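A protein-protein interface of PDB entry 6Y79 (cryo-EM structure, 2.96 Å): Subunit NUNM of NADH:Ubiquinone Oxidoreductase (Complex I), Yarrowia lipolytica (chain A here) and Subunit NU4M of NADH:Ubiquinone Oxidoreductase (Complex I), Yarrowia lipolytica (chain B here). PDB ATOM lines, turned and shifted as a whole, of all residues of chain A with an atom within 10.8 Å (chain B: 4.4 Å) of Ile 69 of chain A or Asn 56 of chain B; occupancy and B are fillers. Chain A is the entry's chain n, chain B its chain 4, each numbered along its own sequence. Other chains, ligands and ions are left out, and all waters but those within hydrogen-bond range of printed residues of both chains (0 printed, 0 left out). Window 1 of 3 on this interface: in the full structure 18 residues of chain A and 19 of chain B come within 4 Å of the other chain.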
ATOM      1  N   LYS A  57     -23.430  14.802  -8.990  1.00  0.00           N
ATOM      2  CA  LYS A  57     -24.098  14.102  -7.908  1.00  0.00           C
ATOM      3  C   LYS A  57     -23.085  13.290  -7.114  1.00  0.00           C
ATOM      4  O   LYS A  57     -22.029  12.910  -7.625  1.00  0.00           O
ATOM      5  CB  LYS A  57     -25.185  13.187  -8.459  1.00  0.00           C
ATOM      6  CG  LYS A  57     -26.271  13.900  -9.220  1.00  0.00           C
ATOM      7  CD  LYS A  57     -27.312  12.915  -9.699  1.00  0.00           C
ATOM      8  CE  LYS A  57     -28.441  13.616 -10.418  1.00  0.00           C
ATOM      9  NZ  LYS A  57     -29.443  12.650 -10.938  1.00  0.00           N
ATOM     10  N   ARG A  59     -21.603   9.958  -5.222  1.00  0.00           N
ATOM     11  CA  ARG A  59     -21.525   8.631  -5.816  1.00  0.00           C
ATOM     12  C   ARG A  59     -22.625   7.723  -5.288  1.00  0.00           C
ATOM     13  O   ARG A  59     -23.188   6.945  -6.058  1.00  0.00           O
ATOM     14  CB  ARG A  59     -20.138   8.017  -5.605  1.00  0.00           C
ATOM     15  CG  ARG A  59     -19.706   7.832  -4.176  1.00  0.00           C
ATOM     16  CD  ARG A  59     -18.313   7.262  -4.118  1.00  0.00           C
ATOM     17  NE  ARG A  59     -18.234   5.889  -4.603  1.00  0.00           N
ATOM     18  CZ  ARG A  59     -18.474   4.818  -3.855  1.00  0.00           C
ATOM     19  NH1 ARG A  59     -18.831   4.956  -2.589  1.00  0.00           N
ATOM     20  NH2 ARG A  59     -18.369   3.604  -4.373  1.00  0.00           N
ATOM     21  N   ASP A  61     -25.519   8.809  -4.541  1.00  0.00           N
ATOM     22  CA  ASP A  61     -26.701   9.288  -5.245  1.00  0.00           C
ATOM     23  C   ASP A  61     -26.869   8.648  -6.614  1.00  0.00           C
ATOM     24  O   ASP A  61     -27.936   8.791  -7.217  1.00  0.00           O
ATOM     25  CB  ASP A  61     -26.656  10.802  -5.465  1.00  0.00           C
ATOM     26  CG  ASP A  61     -26.728  11.598  -4.179  1.00  0.00           C
ATOM     27  OD1 ASP A  61     -27.271  11.086  -3.180  1.00  0.00           O
ATOM     28  OD2 ASP A  61     -26.265  12.760  -4.190  1.00  0.00           O
ATOM     29  N   ILE A  62     -25.836   7.984  -7.137  1.00  0.00           N
ATOM     30  CA  ILE A  62     -25.841   7.455  -8.497  1.00  0.00           C
ATOM     31  C   ILE A  62     -25.834   5.933  -8.435  1.00  0.00           C
ATOM     32  O   ILE A  62     -26.390   5.259  -9.309  1.00  0.00           O
ATOM     33  CB  ILE A  62     -24.641   8.001  -9.297  1.00  0.00           C
ATOM     34  CG1 ILE A  62     -24.627   9.522  -9.250  1.00  0.00           C
ATOM     35  CG2 ILE A  62     -24.714   7.604 -10.754  1.00  0.00           C
ATOM     36  CD1 ILE A  62     -23.429  10.135  -9.914  1.00  0.00           C
ATOM     37  N   LEU A  63     -25.229   5.387  -7.379  1.00  0.00           N
ATOM     38  CA  LEU A  63     -25.263   3.945  -7.163  1.00  0.00           C
ATOM     39  C   LEU A  63     -26.684   3.457  -6.922  1.00  0.00           C
ATOM     40  O   LEU A  63     -27.072   2.387  -7.406  1.00  0.00           O
ATOM     41  CB  LEU A  63     -24.386   3.578  -5.974  1.00  0.00           C
ATOM     42  CG  LEU A  63     -22.878   3.760  -6.021  1.00  0.00           C
ATOM     43  CD1 LEU A  63     -22.312   3.416  -4.675  1.00  0.00           C
ATOM     44  CD2 LEU A  63     -22.259   2.924  -7.083  1.00  0.00           C
ATOM     45  N   ASN A  64     -27.481   4.245  -6.198  1.00  0.00           N
ATOM     46  CA  ASN A  64     -28.867   3.877  -5.940  1.00  0.00           C
ATOM     47  C   ASN A  64     -29.706   3.972  -7.204  1.00  0.00           C
ATOM     48  O   ASN A  64     -30.569   3.121  -7.450  1.00  0.00           O
ATOM     49  CB  ASN A  64     -29.441   4.769  -4.843  1.00  0.00           C
ATOM     50  CG  ASN A  64     -28.867   4.450  -3.481  1.00  0.00           C
ATOM     51  OD1 ASN A  64     -28.796   3.292  -3.084  1.00  0.00           O
ATOM     52  ND2 ASN A  64     -28.451   5.479  -2.761  1.00  0.00           N
ATOM     53  N   GLU A  65     -29.439   4.975  -8.038  1.00  0.00           N
ATOM     54  CA  GLU A  65     -30.160   5.111  -9.296  1.00  0.00           C
ATOM     55  C   GLU A  65     -29.726   4.092 -10.333  1.00  0.00           C
ATOM     56  O   GLU A  65     -30.453   3.870 -11.301  1.00  0.00           O
ATOM     57  CB  GLU A  65     -29.977   6.511  -9.855  1.00  0.00           C
ATOM     58  CG  GLU A  65     -30.631   7.559  -9.011  1.00  0.00           C
ATOM     59  CD  GLU A  65     -30.557   8.921  -9.641  1.00  0.00           C
ATOM     60  OE1 GLU A  65     -29.850   9.060 -10.658  1.00  0.00           O
ATOM     61  OE2 GLU A  65     -31.207   9.853  -9.127  1.00  0.00           O
ATOM     62  N   GLU A  66     -28.553   3.488 -10.174  1.00  0.00           N
ATOM     63  CA  GLU A  66     -28.209   2.376 -11.046  1.00  0.00           C
ATOM     64  C   GLU A  66     -28.791   1.073 -10.519  1.00  0.00           C
ATOM     65  O   GLU A  66     -29.186   0.202 -11.301  1.00  0.00           O
ATOM     66  CB  GLU A  66     -26.702   2.257 -11.195  1.00  0.00           C
ATOM     67  CG  GLU A  66     -26.299   1.458 -12.403  1.00  0.00           C
ATOM     68  CD  GLU A  66     -24.855   1.054 -12.350  1.00  0.00           C
ATOM     69  OE1 GLU A  66     -24.262   1.148 -11.260  1.00  0.00           O
ATOM     70  OE2 GLU A  66     -24.318   0.646 -13.390  1.00  0.00           O
ATOM     71  N   ALA A  67     -28.833   0.909  -9.192  1.00  0.00           N
ATOM     72  CA  ALA A  67     -29.456  -0.277  -8.613  1.00  0.00           C
ATOM     73  C   ALA A  67     -30.952  -0.315  -8.896  1.00  0.00           C
ATOM     74  O   ALA A  67     -31.516  -1.399  -9.071  1.00  0.00           O
ATOM     75  CB  ALA A  67     -29.191  -0.330  -7.109  1.00  0.00           C
ATOM     76  N   LYS A  68     -31.588   0.855  -8.994  1.00  0.00           N
ATOM     77  CA  LYS A  68     -32.988   0.939  -9.396  1.00  0.00           C
ATOM     78  C   LYS A  68     -33.199   0.434 -10.820  1.00  0.00           C
ATOM     79  O   LYS A  68     -34.135  -0.331 -11.085  1.00  0.00           O
ATOM     80  CB  LYS A  68     -33.462   2.383  -9.263  1.00  0.00           C
ATOM     81  CG  LYS A  68     -34.907   2.608  -9.619  1.00  0.00           C
ATOM     82  CD  LYS A  68     -35.826   1.988  -8.589  1.00  0.00           C
ATOM     83  CE  LYS A  68     -37.276   2.121  -9.009  1.00  0.00           C
ATOM     84  NZ  LYS A  68     -37.703   3.541  -9.026  1.00  0.00           N
ATOM     85  N   ILE A  69     -32.316   0.823 -11.742  1.00  0.00           N
ATOM     86  CA  ILE A  69     -32.431   0.405 -13.136  1.00  0.00           C
ATOM     87  C   ILE A  69     -32.098  -1.076 -13.286  1.00  0.00           C
ATOM     88  O   ILE A  69     -32.727  -1.790 -14.074  1.00  0.00           O
ATOM     89  CB  ILE A  69     -31.536   1.304 -14.010  1.00  0.00           C
ATOM     90  CG1 ILE A  69     -32.067   2.732 -13.980  1.00  0.00           C
ATOM     91  CG2 ILE A  69     -31.456   0.822 -15.444  1.00  0.00           C
ATOM     92  CD1 ILE A  69     -31.178   3.719 -14.657  1.00  0.00           C
ATOM     93  N   VAL A  70     -31.140  -1.569 -12.503  1.00  0.00           N
ATOM     94  CA  VAL A  70     -30.792  -2.986 -12.541  1.00  0.00           C
ATOM     95  C   VAL A  70     -31.926  -3.836 -11.982  1.00  0.00           C
ATOM     96  O   VAL A  70     -32.232  -4.912 -12.513  1.00  0.00           O
ATOM     97  CB  VAL A  70     -29.470  -3.210 -11.789  1.00  0.00           C
ATOM     98  CG1 VAL A  70     -29.252  -4.665 -11.436  1.00  0.00           C
ATOM     99  CG2 VAL A  70     -28.344  -2.731 -12.625  1.00  0.00           C
ATOM    100  N   GLN A  71     -32.594  -3.349 -10.932  1.00  0.00           N
ATOM    101  CA  GLN A  71     -33.773  -4.031 -10.414  1.00  0.00           C
ATOM    102  C   GLN A  71     -34.901  -4.036 -11.437  1.00  0.00           C
ATOM    103  O   GLN A  71     -35.551  -5.066 -11.639  1.00  0.00           O
ATOM    104  CB  GLN A  71     -34.220  -3.367  -9.115  1.00  0.00           C
ATOM    105  CG  GLN A  71     -35.328  -4.096  -8.389  1.00  0.00           C
ATOM    106  CD  GLN A  71     -34.941  -5.502  -7.999  1.00  0.00           C
ATOM    107  OE1 GLN A  71     -33.831  -5.747  -7.529  1.00  0.00           O
ATOM    108  NE2 GLN A  71     -35.856  -6.439  -8.196  1.00  0.00           N
ATOM    109  N   ALA A  72     -35.108  -2.913 -12.127  1.00  0.00           N
ATOM    110  CA  ALA A  72     -36.129  -2.836 -13.164  1.00  0.00           C
ATOM    111  C   ALA A  72     -35.816  -3.701 -14.382  1.00  0.00           C
ATOM    112  O   ALA A  72     -36.742  -4.104 -15.090  1.00  0.00           O
ATOM    113  CB  ALA A  72     -36.318  -1.386 -13.595  1.00  0.00           C
ATOM    114  N   LEU A  73     -34.549  -3.986 -14.653  1.00  0.00           N
ATOM    115  CA  LEU A  73     -34.201  -4.864 -15.763  1.00  0.00           C
ATOM    116  C   LEU A  73     -34.213  -6.331 -15.376  1.00  0.00           C
ATOM    117  O   LEU A  73     -34.557  -7.184 -16.202  1.00  0.00           O
ATOM    118  CB  LEU A  73     -32.822  -4.507 -16.306  1.00  0.00           C
ATOM    119  CG  LEU A  73     -32.710  -3.219 -17.102  1.00  0.00           C
ATOM    120  CD1 LEU A  73     -31.274  -2.829 -17.125  1.00  0.00           C
ATOM    121  CD2 LEU A  73     -33.224  -3.414 -18.504  1.00  0.00           C
ATOM    122  N   ASN A  74     -33.850  -6.647 -14.134  1.00  0.00           N
ATOM    123  CA  ASN A  74     -33.987  -8.012 -13.652  1.00  0.00           C
ATOM    124  C   ASN A  74     -35.447  -8.395 -13.492  1.00  0.00           C
ATOM    125  O   ASN A  74     -35.790  -9.568 -13.653  1.00  0.00           O
ATOM    126  CB  ASN A  74     -33.249  -8.180 -12.330  1.00  0.00           C
ATOM    127  CG  ASN A  74     -31.753  -8.194 -12.500  1.00  0.00           C
ATOM    128  OD1 ASN A  74     -31.228  -8.780 -13.444  1.00  0.00           O
ATOM    129  ND2 ASN A  74     -31.054  -7.558 -11.577  1.00  0.00           N
ATOM    130  N   ASN A  75     -36.314  -7.424 -13.188  1.00  0.00           N
ATOM    131  CA  ASN A  75     -37.749  -7.681 -13.178  1.00  0.00           C
ATOM    132  C   ASN A  75     -38.252  -8.065 -14.560  1.00  0.00           C
ATOM    133  O   ASN A  75     -39.052  -8.996 -14.697  1.00  0.00           O
ATOM    134  CB  ASN A  75     -38.504  -6.458 -12.671  1.00  0.00           C
ATOM    135  CG  ASN A  75     -38.376  -6.273 -11.185  1.00  0.00           C
ATOM    136  OD1 ASN A  75     -38.285  -7.238 -10.433  1.00  0.00           O
ATOM    137  ND2 ASN A  75     -38.374  -5.025 -10.749  1.00  0.00           N
ATOM    138  N   GLN A  76     -37.783  -7.372 -15.597  1.00  0.00           N
ATOM    139  CA  GLN A  76     -38.158  -7.715 -16.962  1.00  0.00           C
ATOM    140  C   GLN A  76     -37.573  -9.053 -17.389  1.00  0.00           C
ATOM    141  O   GLN A  76     -38.217  -9.797 -18.135  1.00  0.00           O
ATOM    142  CB  GLN A  76     -37.716  -6.607 -17.912  1.00  0.00           C
ATOM    143  CG  GLN A  76     -38.096  -6.812 -19.362  1.00  0.00           C
ATOM    144  CD  GLN A  76     -39.588  -6.821 -19.583  1.00  0.00           C
ATOM    145  OE1 GLN A  76     -40.319  -6.011 -19.016  1.00  0.00           O
ATOM    146  NE2 GLN A  76     -40.053  -7.738 -20.417  1.00  0.00           N
ATOM    147  N   ARG A  77     -36.383  -9.396 -16.903  1.00  0.00           N
ATOM    148  CA  ARG A  77     -35.814 -10.702 -17.215  1.00  0.00           C
ATOM    149  C   ARG A  77     -36.605 -11.830 -16.557  1.00  0.00           C
ATOM    150  O   ARG A  77     -36.880 -12.858 -17.193  1.00  0.00           O
ATOM    151  CB  ARG A  77     -34.352 -10.749 -16.794  1.00  0.00           C
ATOM    152  CG  ARG A  77     -33.659 -12.008 -17.220  1.00  0.00           C
ATOM    153  CD  ARG A  77     -32.330 -12.152 -16.555  1.00  0.00           C
ATOM    154  NE  ARG A  77     -31.726 -13.426 -16.896  1.00  0.00           N
ATOM    155  CZ  ARG A  77     -31.858 -14.521 -16.166  1.00  0.00           C
ATOM    156  NH1 ARG A  77     -32.570 -14.487 -15.053  1.00  0.00           N
ATOM    157  NH2 ARG A  77     -31.280 -15.647 -16.549  1.00  0.00           N
ATOM    158  N   GLU A  78     -36.992 -11.648 -15.287  1.00  0.00           N
ATOM    159  CA  GLU A  78     -37.856 -12.610 -14.605  1.00  0.00           C
ATOM    160  C   GLU A  78     -39.213 -12.734 -15.280  1.00  0.00           C
ATOM    161  O   GLU A  78     -39.734 -13.848 -15.418  1.00  0.00           O
ATOM    162  CB  GLU A  78     -38.078 -12.203 -13.151  1.00  0.00           C
ATOM    163  CG  GLU A  78     -36.887 -12.297 -12.237  1.00  0.00           C
ATOM    164  CD  GLU A  78     -37.018 -11.344 -11.060  1.00  0.00           C
ATOM    165  OE1 GLU A  78     -38.159 -10.945 -10.746  1.00  0.00           O
ATOM    166  OE2 GLU A  78     -35.985 -10.983 -10.462  1.00  0.00           O
ATOM    167  N   PHE B  53     -22.996   4.652 -14.440  1.00  0.00           N
ATOM    168  CA  PHE B  53     -23.488   5.388 -15.602  1.00  0.00           C
ATOM    169  C   PHE B  53     -24.341   6.553 -15.119  1.00  0.00           C
ATOM    170  O   PHE B  53     -25.355   6.346 -14.450  1.00  0.00           O
ATOM    171  CB  PHE B  53     -24.287   4.465 -16.516  1.00  0.00           C
ATOM    172  CG  PHE B  53     -23.470   3.378 -17.145  1.00  0.00           C
ATOM    173  CD1 PHE B  53     -22.135   3.568 -17.424  1.00  0.00           C
ATOM    174  CD2 PHE B  53     -24.029   2.156 -17.435  1.00  0.00           C
ATOM    175  CE1 PHE B  53     -21.386   2.559 -18.002  1.00  0.00           C
ATOM    176  CE2 PHE B  53     -23.273   1.151 -18.007  1.00  0.00           C
ATOM    177  CZ  PHE B  53     -21.960   1.357 -18.290  1.00  0.00           C
ATOM    178  N   GLN B  54     -23.944   7.774 -15.473  1.00  0.00           N
ATOM    179  CA  GLN B  54     -24.410   8.949 -14.746  1.00  0.00           C
ATOM    180  C   GLN B  54     -25.715   9.528 -15.278  1.00  0.00           C
ATOM    181  O   GLN B  54     -26.620   9.823 -14.490  1.00  0.00           O
ATOM    182  CB  GLN B  54     -23.333  10.039 -14.743  1.00  0.00           C
ATOM    183  CG  GLN B  54     -22.236   9.841 -13.723  1.00  0.00           C
ATOM    184  CD  GLN B  54     -21.183   8.884 -14.205  1.00  0.00           C
ATOM    185  OE1 GLN B  54     -21.220   8.436 -15.346  1.00  0.00           O
ATOM    186  NE2 GLN B  54     -20.236   8.559 -13.344  1.00  0.00           N
ATOM    187  N   PHE B  55     -25.834   9.733 -16.584  1.00  0.00           N
ATOM    188  CA  PHE B  55     -26.983  10.453 -17.132  1.00  0.00           C
ATOM    189  C   PHE B  55     -27.839   9.461 -17.906  1.00  0.00           C
ATOM    190  O   PHE B  55     -27.777   9.379 -19.128  1.00  0.00           O
ATOM    191  CB  PHE B  55     -26.529  11.608 -18.008  1.00  0.00           C
ATOM    192  CG  PHE B  55     -25.809  12.687 -17.259  1.00  0.00           C
ATOM    193  CD1 PHE B  55     -26.104  12.946 -15.935  1.00  0.00           C
ATOM    194  CD2 PHE B  55     -24.825  13.428 -17.869  1.00  0.00           C
ATOM    195  CE1 PHE B  55     -25.436  13.931 -15.242  1.00  0.00           C
ATOM    196  CE2 PHE B  55     -24.159  14.412 -17.177  1.00  0.00           C
ATOM    197  CZ  PHE B  55     -24.466  14.662 -15.868  1.00  0.00           C
ATOM    198  N   ASN B  56     -28.684   8.742 -17.179  1.00  0.00           N
ATOM    199  CA  ASN B  56     -29.452   7.631 -17.720  1.00  0.00           C
ATOM    200  C   ASN B  56     -30.820   8.103 -18.169  1.00  0.00           C
ATOM    201  O   ASN B  56     -31.449   8.927 -17.503  1.00  0.00           O
ATOM    202  CB  ASN B  56     -29.637   6.541 -16.674  1.00  0.00           C
ATOM    203  CG  ASN B  56     -28.363   5.862 -16.319  1.00  0.00           C
ATOM    204  OD1 ASN B  56     -27.611   5.441 -17.186  1.00  0.00           O
ATOM    205  ND2 ASN B  56     -28.105   5.742 -15.029  1.00  0.00           N
ATOM    206  N   PHE B  57     -31.289   7.557 -19.287  1.00  0.00           N
ATOM    207  CA  PHE B  57     -32.674   7.756 -19.670  1.00  0.00           C
ATOM    208  C   PHE B  57     -33.157   6.572 -20.494  1.00  0.00           C
ATOM    209  O   PHE B  57     -32.379   5.910 -21.176  1.00  0.00           O
ATOM    210  CB  PHE B  57     -32.881   9.093 -20.396  1.00  0.00           C
ATOM    211  CG  PHE B  57     -32.178   9.239 -21.700  1.00  0.00           C
ATOM    212  CD1 PHE B  57     -30.893   9.739 -21.753  1.00  0.00           C
ATOM    213  CD2 PHE B  57     -32.843   8.987 -22.885  1.00  0.00           C
ATOM    214  CE1 PHE B  57     -30.261   9.923 -22.957  1.00  0.00           C
ATOM    215  CE2 PHE B  57     -32.216   9.167 -24.093  1.00  0.00           C
ATOM    216  CZ  PHE B  57     -30.926   9.643 -24.129  1.00  0.00           C
ATOM    217  N   LEU B  78     -32.319   1.681 -23.255  1.00  0.00           N
ATOM    218  CA  LEU B  78     -31.609   2.457 -22.252  1.00  0.00           C
ATOM    219  C   LEU B  78     -30.521   3.306 -22.887  1.00  0.00           C
ATOM    220  O   LEU B  78     -29.987   2.971 -23.943  1.00  0.00           O
ATOM    221  CB  LEU B  78     -30.960   1.558 -21.215  1.00  0.00           C
ATOM    222  CG  LEU B  78     -31.709   0.601 -20.323  1.00  0.00           C
ATOM    223  CD1 LEU B  78     -30.668  -0.353 -19.795  1.00  0.00           C
ATOM    224  CD2 LEU B  78     -32.371   1.364 -19.203  1.00  0.00           C
ATOM    225  N   PHE B  79     -30.182   4.406 -22.219  1.00  0.00           N
ATOM    226  CA  PHE B  79     -29.117   5.289 -22.659  1.00  0.00           C
ATOM    227  C   PHE B  79     -28.407   5.864 -21.442  1.00  0.00           C
ATOM    228  O   PHE B  79     -29.037   6.108 -20.414  1.00  0.00           O
ATOM    229  CB  PHE B  79     -29.655   6.418 -23.537  1.00  0.00           C
ATOM    230  CG  PHE B  79     -30.243   5.958 -24.843  1.00  0.00           C
ATOM    231  CD1 PHE B  79     -29.431   5.718 -25.935  1.00  0.00           C
ATOM    232  CD2 PHE B  79     -31.606   5.781 -24.984  1.00  0.00           C
ATOM    233  CE1 PHE B  79     -29.957   5.293 -27.132  1.00  0.00           C
ATOM    234  CE2 PHE B  79     -32.140   5.362 -26.183  1.00  0.00           C
ATOM    235  CZ  PHE B  79     -31.311   5.116 -27.257  1.00  0.00           C
ATOM    236  N   GLY B  80     -27.101   6.072 -21.558  1.00  0.00           N
ATOM    237  CA  GLY B  80     -26.309   6.585 -20.453  1.00  0.00           C
ATOM    238  C   GLY B  80     -24.836   6.465 -20.763  1.00  0.00           C
ATOM    239  O   GLY B  80     -24.427   5.741 -21.669  1.00  0.00           O
ATOM    240  N   LEU B 132     -27.198   1.620 -24.239  1.00  0.00           N
ATOM    241  CA  LEU B 132     -26.905   0.748 -23.116  1.00  0.00           C
ATOM    242  C   LEU B 132     -27.458  -0.661 -23.228  1.00  0.00           C
ATOM    243  O   LEU B 132     -27.141  -1.484 -22.368  1.00  0.00           O
ATOM    244  CB  LEU B 132     -27.409   1.354 -21.807  1.00  0.00           C
ATOM    245  CG  LEU B 132     -26.594   2.456 -21.154  1.00  0.00           C
ATOM    246  CD1 LEU B 132     -27.210   2.805 -19.831  1.00  0.00           C
ATOM    247  CD2 LEU B 132     -25.194   1.982 -20.969  1.00  0.00           C
ATOM    248  N   ILE B 195     -24.876  -2.890 -18.444  1.00  0.00           N
ATOM    249  CA  ILE B 195     -24.677  -2.692 -17.021  1.00  0.00           C
ATOM    250  C   ILE B 195     -24.373  -3.999 -16.311  1.00  0.00           C
ATOM    251  O   ILE B 195     -23.360  -4.126 -15.628  1.00  0.00           O
ATOM    252  CB  ILE B 195     -25.918  -2.020 -16.406  1.00  0.00           C
ATOM    253  CG1 ILE B 195     -26.204  -0.683 -17.076  1.00  0.00           C
ATOM    254  CG2 ILE B 195     -25.687  -1.832 -14.961  1.00  0.00           C
ATOM    255  CD1 ILE B 195     -27.404   0.019 -16.528  1.00  0.00           C
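Ile 69 of chain A touches two residues of chain B.
Asn 56 of chain B touches one residue of chain A.
Phe 57 of chain B touches none of the printed residues of chain A.
Of the printed residues of chain A, Leu 78 of chain B touches Ile 69 and Leu 73.
Of the printed residues of chain B, Val 70 of chain A touches Ile 195 (3.7 Å).
Of the printed residues of chain A, Phe 53 of chain B touches Ile 62.
Of the printed residues of chain B, Glu 66 of chain A touches Ile 195.
Of the printed residues of chain B, Leu 73 of chain A touches Leu 78.
Leu 63 of chain A touches none of the printed residues of chain B.
The nearest residue of chain A that does not touch Asn 56 of chain B is Glu 65 of chain A (4.8 Å).
The nearest printed residue of chain A that does not touch Ile 195 of chain B is Ile 69 of chain A (4.3 Å).
Of the 20 printed residues of chain A, 5 touch a printed residue of chain B.
Among the printed residues, no Asp or Glu carboxylate lies within 4 Å of a Lys or Arg side-chain nitrogen of the other chain.
Among the printed residues, pairs that only touch across the chains: Glu 66 of chain A with Ile 195 of chain B (3.2 Å), Val 70 of chain A with Ile 195 of chain B (3.7 Å), Leu 73 of chain A with Leu 78 of chain B (3.7 Å), Ile 69 of chain A with Asn 56 of chain B (3.7 Å), Ile 69 of chain A with Leu 78 of chain B (3.9 Å) and Ile 62 of chain A with Phe 53 of chain B (3.96 Å).
O of Leu 78 of chain B is in hydrogen-bond range of N of Leu 132 of chain B, at 3.1 Å.
ND2 of Asn 74 of chain A sits at hydrogen-bond distance from O of Val 70 of chain A.
The backbone carbonyl oxygen (O) of Phe 53 of chain B sits at hydrogen-bond distance from the side-chain amide nitrogen (ND2) of Asn 56 of chain B (2.9 Å).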
